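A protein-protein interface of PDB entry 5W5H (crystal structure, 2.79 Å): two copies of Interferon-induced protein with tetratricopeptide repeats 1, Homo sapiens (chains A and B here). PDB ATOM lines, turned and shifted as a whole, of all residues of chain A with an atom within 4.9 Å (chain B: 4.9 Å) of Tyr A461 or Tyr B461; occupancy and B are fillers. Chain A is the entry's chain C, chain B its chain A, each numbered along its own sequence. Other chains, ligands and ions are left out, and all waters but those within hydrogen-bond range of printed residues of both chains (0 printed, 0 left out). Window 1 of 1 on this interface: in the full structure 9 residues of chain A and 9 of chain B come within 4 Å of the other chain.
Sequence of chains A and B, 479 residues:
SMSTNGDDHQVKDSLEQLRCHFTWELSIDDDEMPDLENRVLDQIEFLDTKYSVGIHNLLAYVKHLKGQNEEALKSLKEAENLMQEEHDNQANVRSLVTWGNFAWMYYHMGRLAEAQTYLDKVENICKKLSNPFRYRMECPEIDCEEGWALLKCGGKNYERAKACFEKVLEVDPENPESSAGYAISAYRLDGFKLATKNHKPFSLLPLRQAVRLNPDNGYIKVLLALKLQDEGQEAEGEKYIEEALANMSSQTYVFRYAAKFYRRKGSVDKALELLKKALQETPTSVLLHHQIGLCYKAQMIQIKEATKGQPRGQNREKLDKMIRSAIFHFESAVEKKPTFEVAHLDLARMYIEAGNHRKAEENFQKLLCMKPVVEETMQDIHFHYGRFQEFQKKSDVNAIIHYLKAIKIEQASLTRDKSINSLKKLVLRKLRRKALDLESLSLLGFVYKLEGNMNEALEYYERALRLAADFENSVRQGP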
ATOM      1  N   SER A 442     -31.049 -11.293 -15.332  1.00  0.00           N
ATOM      2  CA  SER A 442     -31.685 -12.554 -15.700  1.00  0.00           C
ATOM      3  C   SER A 442     -33.184 -12.370 -15.904  1.00  0.00           C
ATOM      4  O   SER A 442     -33.779 -12.993 -16.792  1.00  0.00           O
ATOM      5  CB  SER A 442     -31.421 -13.600 -14.621  1.00  0.00           C
ATOM      6  OG  SER A 442     -30.058 -13.593 -14.239  1.00  0.00           O
ATOM      7  N   GLY A 445     -33.862 -10.674 -19.284  1.00  0.00           N
ATOM      8  CA  GLY A 445     -33.761 -11.679 -20.329  1.00  0.00           C
ATOM      9  C   GLY A 445     -34.988 -12.566 -20.382  1.00  0.00           C
ATOM     10  O   GLY A 445     -35.467 -12.920 -21.463  1.00  0.00           O
ATOM     11  N   PHE A 446     -35.515 -12.936 -19.214  1.00  0.00           N
ATOM     12  CA  PHE A 446     -36.761 -13.692 -19.160  1.00  0.00           C
ATOM     13  C   PHE A 446     -37.904 -12.898 -19.780  1.00  0.00           C
ATOM     14  O   PHE A 446     -38.747 -13.458 -20.491  1.00  0.00           O
ATOM     15  CB  PHE A 446     -37.073 -14.056 -17.708  1.00  0.00           C
ATOM     16  CG  PHE A 446     -38.321 -14.873 -17.535  1.00  0.00           C
ATOM     17  CD1 PHE A 446     -38.371 -16.188 -17.963  1.00  0.00           C
ATOM     18  CD2 PHE A 446     -39.435 -14.332 -16.917  1.00  0.00           C
ATOM     19  CE1 PHE A 446     -39.516 -16.942 -17.794  1.00  0.00           C
ATOM     20  CE2 PHE A 446     -40.581 -15.082 -16.744  1.00  0.00           C
ATOM     21  CZ  PHE A 446     -40.621 -16.389 -17.184  1.00  0.00           C
ATOM     22  N   LYS A 449     -37.713 -12.890 -23.532  1.00  0.00           N
ATOM     23  CA  LYS A 449     -38.118 -14.201 -24.026  1.00  0.00           C
ATOM     24  C   LYS A 449     -39.633 -14.283 -24.169  1.00  0.00           C
ATOM     25  O   LYS A 449     -40.150 -14.745 -25.193  1.00  0.00           O
ATOM     26  CB  LYS A 449     -37.598 -15.292 -23.089  1.00  0.00           C
ATOM     27  CG  LYS A 449     -38.078 -16.695 -23.430  1.00  0.00           C
ATOM     28  CD  LYS A 449     -37.477 -17.721 -22.489  1.00  0.00           C
ATOM     29  CE  LYS A 449     -38.513 -18.725 -22.025  1.00  0.00           C
ATOM     30  NZ  LYS A 449     -37.973 -19.629 -20.973  1.00  0.00           N
ATOM     31  N   ALA A 457     -33.013 -11.848 -25.641  1.00  0.00           N
ATOM     32  CA  ALA A 457     -33.129 -12.693 -24.458  1.00  0.00           C
ATOM     33  C   ALA A 457     -31.824 -13.428 -24.183  1.00  0.00           C
ATOM     34  O   ALA A 457     -31.346 -13.464 -23.044  1.00  0.00           O
ATOM     35  CB  ALA A 457     -34.279 -13.683 -24.635  1.00  0.00           C
ATOM     36  N   LEU A 458     -31.234 -14.027 -25.218  1.00  0.00           N
ATOM     37  CA  LEU A 458     -29.952 -14.704 -25.048  1.00  0.00           C
ATOM     38  C   LEU A 458     -28.849 -13.724 -24.676  1.00  0.00           C
ATOM     39  O   LEU A 458     -27.892 -14.099 -23.989  1.00  0.00           O
ATOM     40  CB  LEU A 458     -29.583 -15.455 -26.329  1.00  0.00           C
ATOM     41  CG  LEU A 458     -30.478 -16.643 -26.684  1.00  0.00           C
ATOM     42  CD1 LEU A 458     -30.244 -17.087 -28.117  1.00  0.00           C
ATOM     43  CD2 LEU A 458     -30.230 -17.794 -25.724  1.00  0.00           C
ATOM     44  N   GLU A 459     -28.964 -12.468 -25.109  1.00  0.00           N
ATOM     45  CA  GLU A 459     -27.924 -11.485 -24.821  1.00  0.00           C
ATOM     46  C   GLU A 459     -27.843 -11.198 -23.327  1.00  0.00           C
ATOM     47  O   GLU A 459     -26.759 -11.239 -22.734  1.00  0.00           O
ATOM     48  CB  GLU A 459     -28.188 -10.203 -25.613  1.00  0.00           C
ATOM     49  CG  GLU A 459     -27.075  -9.167 -25.519  1.00  0.00           C
ATOM     50  CD  GLU A 459     -27.193  -8.079 -26.577  1.00  0.00           C
ATOM     51  OE1 GLU A 459     -28.143  -8.133 -27.389  1.00  0.00           O
ATOM     52  OE2 GLU A 459     -26.332  -7.173 -26.600  1.00  0.00           O
ATOM     53  N   TYR A 460     -28.985 -10.919 -22.694  1.00  0.00           N
ATOM     54  CA  TYR A 460     -28.984 -10.591 -21.273  1.00  0.00           C
ATOM     55  C   TYR A 460     -28.767 -11.819 -20.398  1.00  0.00           C
ATOM     56  O   TYR A 460     -28.281 -11.687 -19.270  1.00  0.00           O
ATOM     57  CB  TYR A 460     -30.290  -9.890 -20.893  1.00  0.00           C
ATOM     58  CG  TYR A 460     -30.311  -8.421 -21.258  1.00  0.00           C
ATOM     59  CD1 TYR A 460     -29.718  -7.474 -20.432  1.00  0.00           C
ATOM     60  CD2 TYR A 460     -30.915  -7.981 -22.428  1.00  0.00           C
ATOM     61  CE1 TYR A 460     -29.728  -6.129 -20.761  1.00  0.00           C
ATOM     62  CE2 TYR A 460     -30.931  -6.638 -22.765  1.00  0.00           C
ATOM     63  CZ  TYR A 460     -30.337  -5.717 -21.927  1.00  0.00           C
ATOM     64  OH  TYR A 460     -30.350  -4.380 -22.256  1.00  0.00           O
ATOM     65  N   TYR A 461     -29.119 -13.010 -20.883  1.00  0.00           N
ATOM     66  CA  TYR A 461     -28.759 -14.223 -20.156  1.00  0.00           C
ATOM     67  C   TYR A 461     -27.249 -14.418 -20.143  1.00  0.00           C
ATOM     68  O   TYR A 461     -26.670 -14.763 -19.107  1.00  0.00           O
ATOM     69  CB  TYR A 461     -29.445 -15.442 -20.777  1.00  0.00           C
ATOM     70  CG  TYR A 461     -30.893 -15.666 -20.373  1.00  0.00           C
ATOM     71  CD1 TYR A 461     -31.495 -14.916 -19.367  1.00  0.00           C
ATOM     72  CD2 TYR A 461     -31.653 -16.648 -20.997  1.00  0.00           C
ATOM     73  CE1 TYR A 461     -32.811 -15.133 -19.005  1.00  0.00           C
ATOM     74  CE2 TYR A 461     -32.969 -16.871 -20.640  1.00  0.00           C
ATOM     75  CZ  TYR A 461     -33.542 -16.113 -19.646  1.00  0.00           C
ATOM     76  OH  TYR A 461     -34.853 -16.338 -19.293  1.00  0.00           O
ATOM     77  N   GLU A 462     -26.594 -14.197 -21.284  1.00  0.00           N
ATOM     78  CA  GLU A 462     -25.145 -14.341 -21.340  1.00  0.00           C
ATOM     79  C   GLU A 462     -24.455 -13.278 -20.494  1.00  0.00           C
ATOM     80  O   GLU A 462     -23.468 -13.568 -19.809  1.00  0.00           O
ATOM     81  CB  GLU A 462     -24.676 -14.277 -22.792  1.00  0.00           C
ATOM     82  CG  GLU A 462     -25.048 -15.512 -23.602  1.00  0.00           C
ATOM     83  CD  GLU A 462     -24.862 -15.322 -25.095  1.00  0.00           C
ATOM     84  OE1 GLU A 462     -24.446 -14.222 -25.514  1.00  0.00           O
ATOM     85  OE2 GLU A 462     -25.136 -16.277 -25.851  1.00  0.00           O
ATOM     86  N   ARG A 463     -24.966 -12.044 -20.520  1.00  0.00           N
ATOM     87  CA  ARG A 463     -24.400 -10.991 -19.681  1.00  0.00           C
ATOM     88  C   ARG A 463     -24.484 -11.365 -18.207  1.00  0.00           C
ATOM     89  O   ARG A 463     -23.513 -11.204 -17.458  1.00  0.00           O
ATOM     90  CB  ARG A 463     -25.121  -9.668 -19.947  1.00  0.00           C
ATOM     91  CG  ARG A 463     -24.687  -8.981 -21.235  1.00  0.00           C
ATOM     92  CD  ARG A 463     -25.823  -8.195 -21.872  1.00  0.00           C
ATOM     93  NE  ARG A 463     -26.266  -7.072 -21.045  1.00  0.00           N
ATOM     94  CZ  ARG A 463     -25.962  -5.793 -21.266  1.00  0.00           C
ATOM     95  NH1 ARG A 463     -25.206  -5.437 -22.298  1.00  0.00           N
ATOM     96  NH2 ARG A 463     -26.425  -4.860 -20.445  1.00  0.00           N
ATOM     97  N   ALA A 464     -25.637 -11.878 -17.775  1.00  0.00           N
ATOM     98  CA  ALA A 464     -25.791 -12.279 -16.381  1.00  0.00           C
ATOM     99  C   ALA A 464     -24.865 -13.439 -16.037  1.00  0.00           C
ATOM    100  O   ALA A 464     -24.253 -13.459 -14.961  1.00  0.00           O
ATOM    101  CB  ALA A 464     -27.247 -12.656 -16.102  1.00  0.00           C
ATOM    102  N   LEU A 465     -24.743 -14.415 -16.940  1.00  0.00           N
ATOM    103  CA  LEU A 465     -23.897 -15.574 -16.680  1.00  0.00           C
ATOM    104  C   LEU A 465     -22.425 -15.204 -16.565  1.00  0.00           C
ATOM    105  O   LEU A 465     -21.658 -15.957 -15.957  1.00  0.00           O
ATOM    106  CB  LEU A 465     -24.091 -16.622 -17.777  1.00  0.00           C
ATOM    107  CG  LEU A 465     -25.368 -17.456 -17.662  1.00  0.00           C
ATOM    108  CD1 LEU A 465     -25.616 -18.243 -18.938  1.00  0.00           C
ATOM    109  CD2 LEU A 465     -25.293 -18.395 -16.465  1.00  0.00           C
ATOM    110  N   SER B 442     -23.457 -23.431 -19.022  1.00  0.00           N
ATOM    111  CA  SER B 442     -23.579 -22.234 -19.851  1.00  0.00           C
ATOM    112  C   SER B 442     -22.854 -22.403 -21.182  1.00  0.00           C
ATOM    113  O   SER B 442     -23.362 -21.979 -22.226  1.00  0.00           O
ATOM    114  CB  SER B 442     -23.047 -21.017 -19.095  1.00  0.00           C
ATOM    115  OG  SER B 442     -21.735 -21.247 -18.620  1.00  0.00           O
ATOM    116  N   GLY B 445     -25.085 -24.511 -23.294  1.00  0.00           N
ATOM    117  CA  GLY B 445     -26.134 -23.660 -23.831  1.00  0.00           C
ATOM    118  C   GLY B 445     -25.625 -22.758 -24.937  1.00  0.00           C
ATOM    119  O   GLY B 445     -26.323 -22.508 -25.922  1.00  0.00           O
ATOM    120  N   PHE B 446     -24.396 -22.259 -24.789  1.00  0.00           N
ATOM    121  CA  PHE B 446     -23.780 -21.468 -25.848  1.00  0.00           C
ATOM    122  C   PHE B 446     -23.605 -22.294 -27.117  1.00  0.00           C
ATOM    123  O   PHE B 446     -23.855 -21.805 -28.225  1.00  0.00           O
ATOM    124  CB  PHE B 446     -22.437 -20.920 -25.359  1.00  0.00           C
ATOM    125  CG  PHE B 446     -21.669 -20.161 -26.401  1.00  0.00           C
ATOM    126  CD1 PHE B 446     -22.149 -18.963 -26.902  1.00  0.00           C
ATOM    127  CD2 PHE B 446     -20.452 -20.634 -26.861  1.00  0.00           C
ATOM    128  CE1 PHE B 446     -21.439 -18.260 -27.854  1.00  0.00           C
ATOM    129  CE2 PHE B 446     -19.737 -19.933 -27.811  1.00  0.00           C
ATOM    130  CZ  PHE B 446     -20.232 -18.746 -28.310  1.00  0.00           C
ATOM    131  N   LYS B 449     -26.761 -22.616 -29.016  1.00  0.00           N
ATOM    132  CA  LYS B 449     -27.065 -21.383 -29.734  1.00  0.00           C
ATOM    133  C   LYS B 449     -26.340 -21.344 -31.072  1.00  0.00           C
ATOM    134  O   LYS B 449     -26.922 -20.950 -32.089  1.00  0.00           O
ATOM    135  CB  LYS B 449     -26.689 -20.165 -28.891  1.00  0.00           C
ATOM    136  CG  LYS B 449     -27.073 -18.849 -29.551  1.00  0.00           C
ATOM    137  CD  LYS B 449     -26.715 -17.641 -28.704  1.00  0.00           C
ATOM    138  CE  LYS B 449     -25.245 -17.291 -28.798  1.00  0.00           C
ATOM    139  NZ  LYS B 449     -25.040 -15.832 -28.571  1.00  0.00           N
ATOM    140  N   ALA B 457     -30.839 -23.765 -25.833  1.00  0.00           N
ATOM    141  CA  ALA B 457     -29.891 -22.784 -25.317  1.00  0.00           C
ATOM    142  C   ALA B 457     -30.506 -21.987 -24.173  1.00  0.00           C
ATOM    143  O   ALA B 457     -29.901 -21.840 -23.105  1.00  0.00           O
ATOM    144  CB  ALA B 457     -29.436 -21.856 -26.443  1.00  0.00           C
ATOM    145  N   LEU B 458     -31.716 -21.464 -24.382  1.00  0.00           N
ATOM    146  CA  LEU B 458     -32.425 -20.785 -23.302  1.00  0.00           C
ATOM    147  C   LEU B 458     -32.613 -21.711 -22.107  1.00  0.00           C
ATOM    148  O   LEU B 458     -32.457 -21.290 -20.954  1.00  0.00           O
ATOM    149  CB  LEU B 458     -33.777 -20.278 -23.804  1.00  0.00           C
ATOM    150  CG  LEU B 458     -33.704 -19.182 -24.867  1.00  0.00           C
ATOM    151  CD1 LEU B 458     -35.050 -18.988 -25.543  1.00  0.00           C
ATOM    152  CD2 LEU B 458     -33.225 -17.878 -24.251  1.00  0.00           C
ATOM    153  N   GLU B 459     -32.940 -22.979 -22.363  1.00  0.00           N
ATOM    154  CA  GLU B 459     -33.147 -23.933 -21.279  1.00  0.00           C
ATOM    155  C   GLU B 459     -31.903 -24.045 -20.403  1.00  0.00           C
ATOM    156  O   GLU B 459     -31.987 -23.974 -19.172  1.00  0.00           O
ATOM    157  CB  GLU B 459     -33.528 -25.298 -21.853  1.00  0.00           C
ATOM    158  CG  GLU B 459     -34.824 -25.866 -21.298  1.00  0.00           C
ATOM    159  CD  GLU B 459     -35.294 -27.095 -22.055  1.00  0.00           C
ATOM    160  OE1 GLU B 459     -36.044 -26.940 -23.043  1.00  0.00           O
ATOM    161  OE2 GLU B 459     -34.906 -28.217 -21.665  1.00  0.00           O
ATOM    162  N   TYR B 460     -30.733 -24.214 -21.024  1.00  0.00           N
ATOM    163  CA  TYR B 460     -29.507 -24.391 -20.252  1.00  0.00           C
ATOM    164  C   TYR B 460     -29.058 -23.086 -19.607  1.00  0.00           C
ATOM    165  O   TYR B 460     -28.573 -23.088 -18.470  1.00  0.00           O
ATOM    166  CB  TYR B 460     -28.402 -24.960 -21.138  1.00  0.00           C
ATOM    167  CG  TYR B 460     -28.456 -26.462 -21.266  1.00  0.00           C
ATOM    168  CD1 TYR B 460     -27.933 -27.279 -20.273  1.00  0.00           C
ATOM    169  CD2 TYR B 460     -29.036 -27.066 -22.372  1.00  0.00           C
ATOM    170  CE1 TYR B 460     -27.984 -28.655 -20.378  1.00  0.00           C
ATOM    171  CE2 TYR B 460     -29.091 -28.442 -22.489  1.00  0.00           C
ATOM    172  CZ  TYR B 460     -28.563 -29.233 -21.489  1.00  0.00           C
ATOM    173  OH  TYR B 460     -28.615 -30.606 -21.597  1.00  0.00           O
ATOM    174  N   TYR B 461     -29.198 -21.963 -20.312  1.00  0.00           N
ATOM    175  CA  TYR B 461     -28.877 -20.678 -19.700  1.00  0.00           C
ATOM    176  C   TYR B 461     -29.716 -20.448 -18.451  1.00  0.00           C
ATOM    177  O   TYR B 461     -29.203 -19.991 -17.423  1.00  0.00           O
ATOM    178  CB  TYR B 461     -29.092 -19.542 -20.704  1.00  0.00           C
ATOM    179  CG  TYR B 461     -27.994 -19.366 -21.741  1.00  0.00           C
ATOM    180  CD1 TYR B 461     -26.797 -20.070 -21.659  1.00  0.00           C
ATOM    181  CD2 TYR B 461     -28.155 -18.479 -22.799  1.00  0.00           C
ATOM    182  CE1 TYR B 461     -25.803 -19.901 -22.601  1.00  0.00           C
ATOM    183  CE2 TYR B 461     -27.167 -18.305 -23.744  1.00  0.00           C
ATOM    184  CZ  TYR B 461     -25.992 -19.017 -23.641  1.00  0.00           C
ATOM    185  OH  TYR B 461     -24.999 -18.848 -24.580  1.00  0.00           O
ATOM    186  N   GLU B 462     -31.010 -20.769 -18.517  1.00  0.00           N
ATOM    187  CA  GLU B 462     -31.870 -20.613 -17.350  1.00  0.00           C
ATOM    188  C   GLU B 462     -31.486 -21.592 -16.248  1.00  0.00           C
ATOM    189  O   GLU B 462     -31.419 -21.215 -15.073  1.00  0.00           O
ATOM    190  CB  GLU B 462     -33.331 -20.794 -17.757  1.00  0.00           C
ATOM    191  CG  GLU B 462     -33.847 -19.678 -18.647  1.00  0.00           C
ATOM    192  CD  GLU B 462     -35.220 -19.966 -19.211  1.00  0.00           C
ATOM    193  OE1 GLU B 462     -35.787 -21.030 -18.887  1.00  0.00           O
ATOM    194  OE2 GLU B 462     -35.729 -19.128 -19.983  1.00  0.00           O
ATOM    195  N   ARG B 463     -31.230 -22.855 -16.605  1.00  0.00           N
ATOM    196  CA  ARG B 463     -30.796 -23.824 -15.605  1.00  0.00           C
ATOM    197  C   ARG B 463     -29.500 -23.376 -14.942  1.00  0.00           C
ATOM    198  O   ARG B 463     -29.343 -23.494 -13.721  1.00  0.00           O
ATOM    199  CB  ARG B 463     -30.621 -25.204 -16.243  1.00  0.00           C
ATOM    200  CG  ARG B 463     -30.426 -26.322 -15.223  1.00  0.00           C
ATOM    201  CD  ARG B 463     -29.801 -27.569 -15.832  1.00  0.00           C
ATOM    202  NE  ARG B 463     -30.707 -28.275 -16.735  1.00  0.00           N
ATOM    203  CZ  ARG B 463     -30.473 -29.487 -17.234  1.00  0.00           C
ATOM    204  NH1 ARG B 463     -29.361 -30.139 -16.916  1.00  0.00           N
ATOM    205  NH2 ARG B 463     -31.355 -30.051 -18.048  1.00  0.00           N
ATOM    206  N   ALA B 464     -28.560 -22.855 -15.730  1.00  0.00           N
ATOM    207  CA  ALA B 464     -27.305 -22.376 -15.164  1.00  0.00           C
ATOM    208  C   ALA B 464     -27.528 -21.151 -14.286  1.00  0.00           C
ATOM    209  O   ALA B 464     -26.899 -21.015 -13.231  1.00  0.00           O
ATOM    210  CB  ALA B 464     -26.315 -22.061 -16.284  1.00  0.00           C
ATOM    211  N   LEU B 465     -28.421 -20.251 -14.701  1.00  0.00           N
ATOM    212  CA  LEU B 465     -28.685 -19.046 -13.922  1.00  0.00           C
ATOM    213  C   LEU B 465     -29.371 -19.349 -12.595  1.00  0.00           C
ATOM    214  O   LEU B 465     -29.390 -18.483 -11.712  1.00  0.00           O
ATOM    215  CB  LEU B 465     -29.533 -18.072 -14.738  1.00  0.00           C
ATOM    216  CG  LEU B 465     -28.763 -17.225 -15.752  1.00  0.00           C
ATOM    217  CD1 LEU B 465     -29.718 -16.596 -16.753  1.00  0.00           C
ATOM    218  CD2 LEU B 465     -27.949 -16.148 -15.047  1.00  0.00           C
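The side-chain carboxylate (OE2) of Glu A462 lies within salt-bridge range of the side-chain amino group (NZ) of Lys B449 (2.8 Å). OE2 of Glu A462 is in hydrogen-bond range of OH of Tyr B461 (2.9 Å). The side-chain amino group (NZ) of Lys A449 lies within salt-bridge range of the side-chain carboxylate (OE2) of Glu B462. The side-chain hydroxyl (OH) of Tyr A461 lies within hydrogen-bond range of the side-chain carboxylate (OE2) of Glu B462 (3.0 Å).
The side-chain hydroxyl of Tyr A461 lies close to the backbone NH of Phe A446 (3.5 Å). The backbone NH of Phe B446 sits close to the side-chain hydroxyl of Tyr B461 (3.5 Å).
Lys B449 touches Leu A458 (CD to CD1, 3.6 Å). Leu A458 touches Leu B458 (CD2 to CD2, 3.3 Å). Tyr B461 touches Leu A458 (CD2 to CD2, 3.7 Å). CE2 of Tyr A461 touches CD2 of Leu B458, at 3.8 Å. Tyr B461 touches Tyr A461 (CD2 to CB, 3.9 Å). CD2 of Leu B465 touches CB of Ala A464, at 3.7 Å. Ser B442 touches Leu A465 (CB to CD1, 3.8 Å). CD1 of Leu A465 touches CD1 of Tyr B461 (3.5 Å). Ala B464 touches Leu A465. Leu A465 touches Leu B465 (CD2 to CG, 3.7 Å).
Of the printed residues of chain B, Tyr A461 touches Leu B458 (3.8 Å), Tyr B461 (3.9 Å), Glu B462 (3.0 Å) and Leu B465 (3.6 Å). Tyr B461 touches four residues of chain A. Of the printed residues of chain B, Ala A464 touches Leu B465. Of the printed residues of chain B, Lys A449 touches Glu B462. The nearest printed residue of chain B that does not touch Tyr A461 is Ala B457 (5.9 Å). The nearest printed residue of chain B that does not touch Lys A449 is Leu B458 (4.1 Å).
Of the 13 printed residues of chain B, 7 touch a printed residue of chain A. Hydrophobic or aromatic side chains of chain B that line the printed part of chain A: Leu B458, Tyr B461, Ala B464 and Leu B465. Of the 13 printed residues of chain A, 7 touch a printed residue of chain B. Among the printed residues, 16 pairs touch across the chains. Among the printed residues, Asp or Glu carboxylates within 4 Å of a Lys or Arg side-chain nitrogen of the other chain: Lys A449 with Glu B462 and Glu A462 with Lys B449.
Ser A442 touches Leu B465, and with the chains exchanged Leu A465 touches Ser B442. Leu A458 touches Lys B449, but with the chains exchanged Lys A449 does not touch Leu B458 (4.1 Å). Tyr A461 touches Glu B462, and with the chains exchanged Glu A462 touches Tyr B461. Ala A464 touches Leu B465, and with the chains exchanged Leu A465 touches Ala B464.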
